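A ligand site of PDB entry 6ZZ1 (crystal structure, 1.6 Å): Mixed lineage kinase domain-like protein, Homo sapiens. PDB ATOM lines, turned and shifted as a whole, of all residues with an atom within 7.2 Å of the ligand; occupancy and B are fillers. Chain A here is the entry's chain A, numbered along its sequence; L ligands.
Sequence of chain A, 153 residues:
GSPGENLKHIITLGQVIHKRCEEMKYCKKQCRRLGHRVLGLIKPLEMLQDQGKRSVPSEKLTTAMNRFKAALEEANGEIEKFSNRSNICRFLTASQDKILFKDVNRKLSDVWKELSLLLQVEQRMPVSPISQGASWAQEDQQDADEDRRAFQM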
ATOM      1  N   LYS A  25      10.967 -16.643 -13.068  1.00  0.00           N
ATOM      2  CA  LYS A  25      10.990 -16.341 -11.643  1.00  0.00           C
ATOM      3  C   LYS A  25      10.380 -17.434 -10.758  1.00  0.00           C
ATOM      4  O   LYS A  25      10.657 -17.489  -9.548  1.00  0.00           O
ATOM      5  CB  LYS A  25      10.283 -14.988 -11.382  1.00  0.00           C
ATOM      6  CG  LYS A  25      11.047 -13.855 -12.046  1.00  0.00           C
ATOM      7  CD  LYS A  25      10.328 -12.519 -11.958  1.00  0.00           C
ATOM      8  CE  LYS A  25      10.917 -11.530 -12.934  1.00  0.00           C
ATOM      9  NZ  LYS A  25      12.413 -11.429 -12.813  1.00  0.00           N
ATOM     10  N   TYR A  26       9.542 -18.271 -11.345  1.00  0.00           N
ATOM     11  CA  TYR A  26       8.830 -19.317 -10.621  1.00  0.00           C
ATOM     12  C   TYR A  26       9.112 -20.665 -11.250  1.00  0.00           C
ATOM     13  O   TYR A  26       9.438 -20.743 -12.452  1.00  0.00           O
ATOM     14  CB  TYR A  26       7.311 -19.032 -10.614  1.00  0.00           C
ATOM     15  CG  TYR A  26       6.981 -17.578 -10.308  1.00  0.00           C
ATOM     16  CD1 TYR A  26       7.214 -17.053  -9.044  1.00  0.00           C
ATOM     17  CD2 TYR A  26       6.547 -16.718 -11.305  1.00  0.00           C
ATOM     18  CE1 TYR A  26       6.956 -15.708  -8.761  1.00  0.00           C
ATOM     19  CE2 TYR A  26       6.285 -15.375 -11.034  1.00  0.00           C
ATOM     20  CZ  TYR A  26       6.495 -14.874  -9.760  1.00  0.00           C
ATOM     21  OH  TYR A  26       6.235 -13.542  -9.488  1.00  0.00           O
ATOM     22  N   CYS A  27       9.036 -21.737 -10.433  1.00  0.00           N
ATOM     23  CA  CYS A  27       9.324 -23.102 -10.903  1.00  0.00           C
ATOM     24  C   CYS A  27      10.719 -23.191 -11.561  1.00  0.00           C
ATOM     25  O   CYS A  27      10.860 -23.749 -12.662  1.00  0.00           O
ATOM     26  CB  CYS A  27       8.220 -23.659 -11.786  1.00  0.00           C
ATOM     27  SG  CYS A  27       6.670 -24.034 -10.911  1.00  0.00           S
ATOM     28  N   LYS A  28      11.727 -22.600 -10.893  1.00  0.00           N
ATOM     29  CA  LYS A  28      13.090 -22.478 -11.408  1.00  0.00           C
ATOM     30  C   LYS A  28      13.752 -23.816 -11.747  1.00  0.00           C
ATOM     31  O   LYS A  28      14.425 -23.891 -12.776  1.00  0.00           O
ATOM     32  CB  LYS A  28      13.975 -21.653 -10.473  1.00  0.00           C
ATOM     33  CG  LYS A  28      13.559 -20.185 -10.390  1.00  0.00           C
ATOM     34  CD  LYS A  28      14.447 -19.395  -9.399  1.00  0.00           C
ATOM     35  CE  LYS A  28      14.037 -17.938  -9.346  1.00  0.00           C
ATOM     36  NZ  LYS A  28      14.929 -17.109  -8.497  1.00  0.00           N
ATOM     37  N   GLN A  30      12.286 -26.721 -12.735  1.00  0.00           N
ATOM     38  CA  GLN A  30      11.673 -27.238 -13.954  1.00  0.00           C
ATOM     39  C   GLN A  30      11.990 -26.378 -15.190  1.00  0.00           C
ATOM     40  O   GLN A  30      12.227 -26.936 -16.277  1.00  0.00           O
ATOM     41  CB  GLN A  30      10.169 -27.399 -13.801  1.00  0.00           C
ATOM     42  CG  GLN A  30       9.812 -28.470 -12.789  1.00  0.00           C
ATOM     43  CD  GLN A  30       8.353 -28.421 -12.442  1.00  0.00           C
ATOM     44  OE1 GLN A  30       7.556 -29.127 -13.040  1.00  0.00           O
ATOM     45  NE2 GLN A  30       7.955 -27.586 -11.443  1.00  0.00           N
ATOM     46  N   ASN A  84       3.611 -15.403 -17.016  1.00  0.00           N
ATOM     47  CA  ASN A  84       2.547 -14.786 -16.251  1.00  0.00           C
ATOM     48  C   ASN A  84       2.307 -15.659 -14.999  1.00  0.00           C
ATOM     49  O   ASN A  84       1.833 -16.791 -15.119  1.00  0.00           O
ATOM     50  CB  ASN A  84       1.291 -14.725 -17.089  1.00  0.00           C
ATOM     51  CG  ASN A  84       0.192 -13.940 -16.428  1.00  0.00           C
ATOM     52  OD1 ASN A  84      -0.655 -14.481 -15.708  1.00  0.00           O
ATOM     53  ND2 ASN A  84       0.184 -12.629 -16.647  1.00  0.00           N
ATOM     54  N   ARG A  85       2.640 -15.139 -13.797  1.00  0.00           N
ATOM     55  CA  ARG A  85       2.483 -15.862 -12.534  1.00  0.00           C
ATOM     56  C   ARG A  85       1.115 -16.535 -12.355  1.00  0.00           C
ATOM     57  O   ARG A  85       1.055 -17.676 -11.900  1.00  0.00           O
ATOM     58  CB  ARG A  85       2.771 -14.942 -11.348  1.00  0.00           C
ATOM     59  CG  ARG A  85       2.661 -15.646  -9.984  1.00  0.00           C
ATOM     60  CD  ARG A  85       3.022 -14.745  -8.818  1.00  0.00           C
ATOM     61  NE  ARG A  85       2.261 -13.496  -8.809  1.00  0.00           N
ATOM     62  CZ  ARG A  85       2.814 -12.286  -8.794  1.00  0.00           C
ATOM     63  NH1 ARG A  85       4.132 -12.146  -8.749  1.00  0.00           N
ATOM     64  NH2 ARG A  85       2.041 -11.204  -8.793  1.00  0.00           N
ATOM     65  N   SER A  86       0.014 -15.825 -12.680  1.00  0.00           N
ATOM     66  CA  SER A  86      -1.344 -16.369 -12.561  1.00  0.00           C
ATOM     67  C   SER A  86      -1.545 -17.678 -13.363  1.00  0.00           C
ATOM     68  O   SER A  86      -2.202 -18.600 -12.878  1.00  0.00           O
ATOM     69  CB  SER A  86      -2.381 -15.324 -12.950  1.00  0.00           C
ATOM     70  OG  SER A  86      -3.540 -15.889 -13.558  1.00  0.00           O
ATOM     71  N   ASN A  87      -0.988 -17.752 -14.595  1.00  0.00           N
ATOM     72  CA  ASN A  87      -1.122 -18.947 -15.429  1.00  0.00           C
ATOM     73  C   ASN A  87      -0.421 -20.143 -14.797  1.00  0.00           C
ATOM     74  O   ASN A  87      -0.949 -21.252 -14.888  1.00  0.00           O
ATOM     75  CB  ASN A  87      -0.579 -18.711 -16.831  1.00  0.00           C
ATOM     76  CG  ASN A  87      -1.422 -17.744 -17.638  1.00  0.00           C
ATOM     77  OD1 ASN A  87      -2.624 -17.569 -17.385  1.00  0.00           O
ATOM     78  ND2 ASN A  87      -0.795 -17.096 -18.612  1.00  0.00           N
ATOM     79  N   ILE A  88       0.762 -19.896 -14.148  1.00  0.00           N
ATOM     80  CA  ILE A  88       1.479 -20.946 -13.416  1.00  0.00           C
ATOM     81  C   ILE A  88       0.570 -21.453 -12.268  1.00  0.00           C
ATOM     82  O   ILE A  88       0.354 -22.654 -12.137  1.00  0.00           O
ATOM     83  CB  ILE A  88       2.849 -20.452 -12.826  1.00  0.00           C
ATOM     84  CG1 ILE A  88       3.880 -20.274 -13.918  1.00  0.00           C
ATOM     85  CG2 ILE A  88       3.352 -21.399 -11.696  1.00  0.00           C
ATOM     86  CD1 ILE A  88       5.356 -19.969 -13.401  1.00  0.00           C
ATOM     87  N   CYS A  89       0.059 -20.501 -11.423  1.00  0.00           N
ATOM     88  CA  CYS A  89      -0.761 -20.888 -10.285  1.00  0.00           C
ATOM     89  C   CYS A  89      -2.003 -21.639 -10.704  1.00  0.00           C
ATOM     90  O   CYS A  89      -2.245 -22.720 -10.193  1.00  0.00           O
ATOM     91  CB  CYS A  89      -1.064 -19.694  -9.378  1.00  0.00           C
ATOM     92  SG  CYS A  89       0.404 -18.961  -8.624  1.00  0.00           S
ATOM     93  N   ARG A  90      -2.680 -21.160 -11.737  1.00  0.00           N
ATOM     94  CA  ARG A  90      -3.833 -21.863 -12.289  1.00  0.00           C
ATOM     95  C   ARG A  90      -3.470 -23.267 -12.801  1.00  0.00           C
ATOM     96  O   ARG A  90      -4.071 -24.242 -12.355  1.00  0.00           O
ATOM     97  CB  ARG A  90      -4.544 -20.992 -13.334  1.00  0.00           C
ATOM     98  CG  ARG A  90      -5.195 -19.788 -12.678  1.00  0.00           C
ATOM     99  CD  ARG A  90      -5.999 -18.970 -13.648  1.00  0.00           C
ATOM    100  NE  ARG A  90      -7.090 -19.756 -14.237  1.00  0.00           N
ATOM    101  CZ  ARG A  90      -7.602 -19.555 -15.439  1.00  0.00           C
ATOM    102  NH1 ARG A  90      -8.581 -20.326 -15.894  1.00  0.00           N
ATOM    103  NH2 ARG A  90      -7.131 -18.583 -16.217  1.00  0.00           N
ATOM    104  N   LEU A  92      -0.873 -25.273 -12.052  1.00  0.00           N
ATOM    105  CA  LEU A  92      -0.432 -26.188 -10.997  1.00  0.00           C
ATOM    106  C   LEU A  92      -1.552 -26.635 -10.076  1.00  0.00           C
ATOM    107  O   LEU A  92      -1.599 -27.799  -9.682  1.00  0.00           O
ATOM    108  CB  LEU A  92       0.743 -25.583 -10.212  1.00  0.00           C
ATOM    109  CG  LEU A  92       2.057 -25.456 -11.019  1.00  0.00           C
ATOM    110  CD1 LEU A  92       3.099 -24.735 -10.232  1.00  0.00           C
ATOM    111  CD2 LEU A  92       2.586 -26.815 -11.403  1.00  0.00           C
ATOM    112  N   THR A  93      -2.499 -25.758  -9.786  1.00  0.00           N
ATOM    113  CA  THR A  93      -3.658 -26.107  -8.949  1.00  0.00           C
ATOM    114  C   THR A  93      -4.548 -27.188  -9.633  1.00  0.00           C
ATOM    115  O   THR A  93      -5.131 -28.038  -8.965  1.00  0.00           O
ATOM    116  CB  THR A  93      -4.407 -24.832  -8.543  1.00  0.00           C
ATOM    117  OG1 THR A  93      -4.678 -24.087  -9.717  1.00  0.00           O
ATOM    118  CG2 THR A  93      -3.592 -23.931  -7.620  1.00  0.00           C
ATOM    119  N   LYS A  98       1.876 -32.020 -10.687  1.00  0.00           N
ATOM    120  CA  LYS A  98       2.522 -30.726 -10.512  1.00  0.00           C
ATOM    121  C   LYS A  98       3.747 -30.524 -11.430  1.00  0.00           C
ATOM    122  O   LYS A  98       4.553 -29.632 -11.193  1.00  0.00           O
ATOM    123  CB  LYS A  98       2.885 -30.453  -9.042  1.00  0.00           C
ATOM    124  CG  LYS A  98       1.757 -30.833  -8.046  1.00  0.00           C
ATOM    125  CD  LYS A  98       0.449 -30.091  -8.340  1.00  0.00           C
ATOM    126  CE  LYS A  98      -0.720 -30.664  -7.579  1.00  0.00           C
ATOM    127  NZ  LYS A  98      -1.960 -29.874  -7.827  1.00  0.00           N
ATOM    128  N   ALA A 144       9.898 -31.036  -9.847  1.00  0.00           N
ATOM    129  CA  ALA A 144       8.556 -30.568  -9.436  1.00  0.00           C
ATOM    130  C   ALA A 144       8.447 -30.531  -7.914  1.00  0.00           C
ATOM    131  O   ALA A 144       7.816 -29.630  -7.376  1.00  0.00           O
ATOM    132  CB  ALA A 144       7.465 -31.464  -9.994  1.00  0.00           C
ATOM    133  N   GLU A 146      11.096 -30.203  -5.751  1.00  0.00           N
ATOM    134  CA  GLU A 146      11.980 -29.124  -5.305  1.00  0.00           C
ATOM    135  C   GLU A 146      11.266 -27.779  -5.483  1.00  0.00           C
ATOM    136  O   GLU A 146      11.312 -26.955  -4.587  1.00  0.00           O
ATOM    137  CB  GLU A 146      13.342 -29.145  -6.045  1.00  0.00           C
ATOM    138  CG  GLU A 146      14.219 -30.341  -5.717  1.00  0.00           C
ATOM    139  CD  GLU A 146      15.619 -30.342  -6.315  1.00  0.00           C
ATOM    140  OE1 GLU A 146      16.240 -31.419  -6.380  1.00  0.00           O
ATOM    141  OE2 GLU A 146      16.097 -29.254  -6.708  1.00  0.00           O
ATOM    142  N   ASP A 147      10.566 -27.592  -6.645  1.00  0.00           N
ATOM    143  CA  ASP A 147       9.795 -26.370  -6.921  1.00  0.00           C
ATOM    144  C   ASP A 147       8.603 -26.173  -5.969  1.00  0.00           C
ATOM    145  O   ASP A 147       8.392 -25.068  -5.476  1.00  0.00           O
ATOM    146  CB  ASP A 147       9.344 -26.323  -8.396  1.00  0.00           C
ATOM    147  CG  ASP A 147      10.486 -25.988  -9.352  1.00  0.00           C
ATOM    148  OD1 ASP A 147      11.493 -25.425  -8.897  1.00  0.00           O
ATOM    149  OD2 ASP A 147      10.343 -26.256 -10.579  1.00  0.00           O
ATOM    150  N   ARG A 148       7.877 -27.259  -5.677  1.00  0.00           N
ATOM    151  CA  ARG A 148       6.734 -27.210  -4.771  1.00  0.00           C
ATOM    152  C   ARG A 148       7.194 -26.830  -3.363  1.00  0.00           C
ATOM    153  O   ARG A 148       6.589 -25.941  -2.779  1.00  0.00           O
ATOM    154  CB  ARG A 148       6.013 -28.555  -4.772  1.00  0.00           C
ATOM    155  CG  ARG A 148       4.616 -28.505  -4.205  1.00  0.00           C
ATOM    156  CD  ARG A 148       3.987 -29.882  -4.305  1.00  0.00           C
ATOM    157  NE  ARG A 148       2.671 -29.983  -3.666  1.00  0.00           N
ATOM    158  CZ  ARG A 148       1.535 -29.444  -4.112  1.00  0.00           C
ATOM    159  NH1 ARG A 148       0.412 -29.593  -3.422  1.00  0.00           N
ATOM    160  NH2 ARG A 148       1.538 -28.720  -5.228  1.00  0.00           N
ATOM    161  N   ARG A 149       8.331 -27.418  -2.895  1.00  0.00           N
ATOM    162  CA  ARG A 149       8.984 -27.122  -1.604  1.00  0.00           C
ATOM    163  C   ARG A 149       9.451 -25.665  -1.494  1.00  0.00           C
ATOM    164  O   ARG A 149       9.277 -25.038  -0.453  1.00  0.00           O
ATOM    165  CB  ARG A 149      10.196 -28.043  -1.372  1.00  0.00           C
ATOM    166  CG  ARG A 149       9.851 -29.395  -0.794  1.00  0.00           C
ATOM    167  CD  ARG A 149      11.110 -30.065  -0.255  1.00  0.00           C
ATOM    168  NE  ARG A 149      12.061 -30.432  -1.307  1.00  0.00           N
ATOM    169  CZ  ARG A 149      12.042 -31.598  -1.949  1.00  0.00           C
ATOM    170  NH1 ARG A 149      12.954 -31.860  -2.884  1.00  0.00           N
ATOM    171  NH2 ARG A 149      11.114 -32.502  -1.688  1.00  0.00           N
ATOM    172  N   ALA A 150      10.065 -25.121  -2.576  1.00  0.00           N
ATOM    173  CA  ALA A 150      10.508 -23.729  -2.568  1.00  0.00           C
ATOM    174  C   ALA A 150       9.299 -22.802  -2.374  1.00  0.00           C
ATOM    175  O   ALA A 150       9.389 -21.827  -1.621  1.00  0.00           O
ATOM    176  CB  ALA A 150      11.193 -23.406  -3.887  1.00  0.00           C
ATOM    177  N   PHE A 151       8.159 -23.151  -3.014  1.00  0.00           N
ATOM    178  CA  PHE A 151       6.905 -22.390  -2.969  1.00  0.00           C
ATOM    179  C   PHE A 151       6.214 -22.505  -1.605  1.00  0.00           C
ATOM    180  O   PHE A 151       5.599 -21.549  -1.170  1.00  0.00           O
ATOM    181  CB  PHE A 151       5.945 -22.876  -4.080  1.00  0.00           C
ATOM    182  CG  PHE A 151       4.535 -22.318  -4.014  1.00  0.00           C
ATOM    183  CD1 PHE A 151       4.269 -21.001  -4.383  1.00  0.00           C
ATOM    184  CD2 PHE A 151       3.495 -23.083  -3.528  1.00  0.00           C
ATOM    185  CE1 PHE A 151       2.992 -20.486  -4.285  1.00  0.00           C
ATOM    186  CE2 PHE A 151       2.218 -22.567  -3.430  1.00  0.00           C
ATOM    187  CZ  PHE A 151       1.969 -21.269  -3.824  1.00  0.00           C
ATOM    188  N   GLN A 152       6.293 -23.675  -0.980  1.00  0.00           N
ATOM    189  CA  GLN A 152       5.599 -23.912   0.290  1.00  0.00           C
ATOM    190  C   GLN A 152       6.287 -23.315   1.547  1.00  0.00           C
ATOM    191  O   GLN A 152       5.672 -23.388   2.626  1.00  0.00           O
ATOM    192  CB  GLN A 152       5.351 -25.421   0.478  1.00  0.00           C
ATOM    193  CG  GLN A 152       4.277 -25.946  -0.456  1.00  0.00           C
ATOM    194  CD  GLN A 152       4.111 -27.461  -0.406  1.00  0.00           C
ATOM    195  OE1 GLN A 152       4.972 -28.195   0.090  1.00  0.00           O
ATOM    196  NE2 GLN A 152       2.994 -27.960  -0.926  1.00  0.00           N
HETATM  197  N1  LIG L   1       2.723 -20.366  -8.328  1.00  0.00           N
HETATM  198  C1  LIG L   1       4.457 -22.205  -7.862  1.00  0.00           C
HETATM  199  C2  LIG L   1       1.351 -20.342  -8.118  1.00  0.00           C
HETATM  200  C3  LIG L   1       3.556 -19.326  -8.925  1.00  0.00           C
HETATM  201  C4  LIG L   1       4.346 -17.323  -5.986  1.00  0.00           C
HETATM  202  C5  LIG L   1       3.172 -21.585  -7.844  1.00  0.00           C
HETATM  203  N2  LIG L   1       4.445 -23.516  -7.352  1.00  0.00           N
HETATM  204  C6  LIG L   1       5.691 -24.281  -7.424  1.00  0.00           C
HETATM  205  O1  LIG L   1       5.494 -21.713  -8.298  1.00  0.00           O
HETATM  206  O2  LIG L   1       3.699 -18.201  -8.098  1.00  0.00           O
HETATM  207  C7  LIG L   1       4.588 -18.397  -7.011  1.00  0.00           C
HETATM  208  O3  LIG L   1       4.787 -16.077  -6.473  1.00  0.00           O
HETATM  209  C8  LIG L   1       4.585 -15.024  -5.540  1.00  0.00           C
HETATM  210  N3  LIG L   1       0.934 -21.451  -7.516  1.00  0.00           N
HETATM  211  C9  LIG L   1       2.064 -22.200  -7.367  1.00  0.00           C
HETATM  212  N4  LIG L   1       2.112 -23.488  -6.849  1.00  0.00           N
HETATM  213  C10 LIG L   1       3.332 -24.168  -6.822  1.00  0.00           C
HETATM  214  O4  LIG L   1       3.420 -25.298  -6.348  1.00  0.00           O
HETATM  215  C11 LIG L   1       0.904 -24.174  -6.366  1.00  0.00           C
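Merely in contact with the ligand: Tyr 26, Arg 85, Leu 92, Asp 147, Ile 88 and Phe 151. Hydrophobic or aromatic side chains within 4 Å of the ligand: Tyr 26, Ile 88, Leu 92 and Phe 151. The nearest printed residue that does not touch the ligand is Arg 148 (4.04 Å).
The side-chain sulfur (SG) of Cys 89 is bonded to a carbon (C2) of the ligand (1.7 Å). The side-chain sulfur (SG) of Cys 27 lies close to an oxygen (O1) of the ligand.
The backbone carbonyl oxygen (O) of Cys 89 is in hydrogen-bond range of the side-chain hydroxyl (OG1) of Thr 93 (2.8 Å). OH of Tyr 26 is in hydrogen-bond range of NH1 of Arg 85 (2.6 Å). The backbone carbonyl oxygen (O) of Leu 92 sits at hydrogen-bond distance from the side-chain amino group (NZ) of Lys 98. OD2 of Asp 147 sits at hydrogen-bond distance from NE2 of Gln 30. N of Lys 28 sits at hydrogen-bond distance from OD1 of Asp 147 (3.5 Å).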
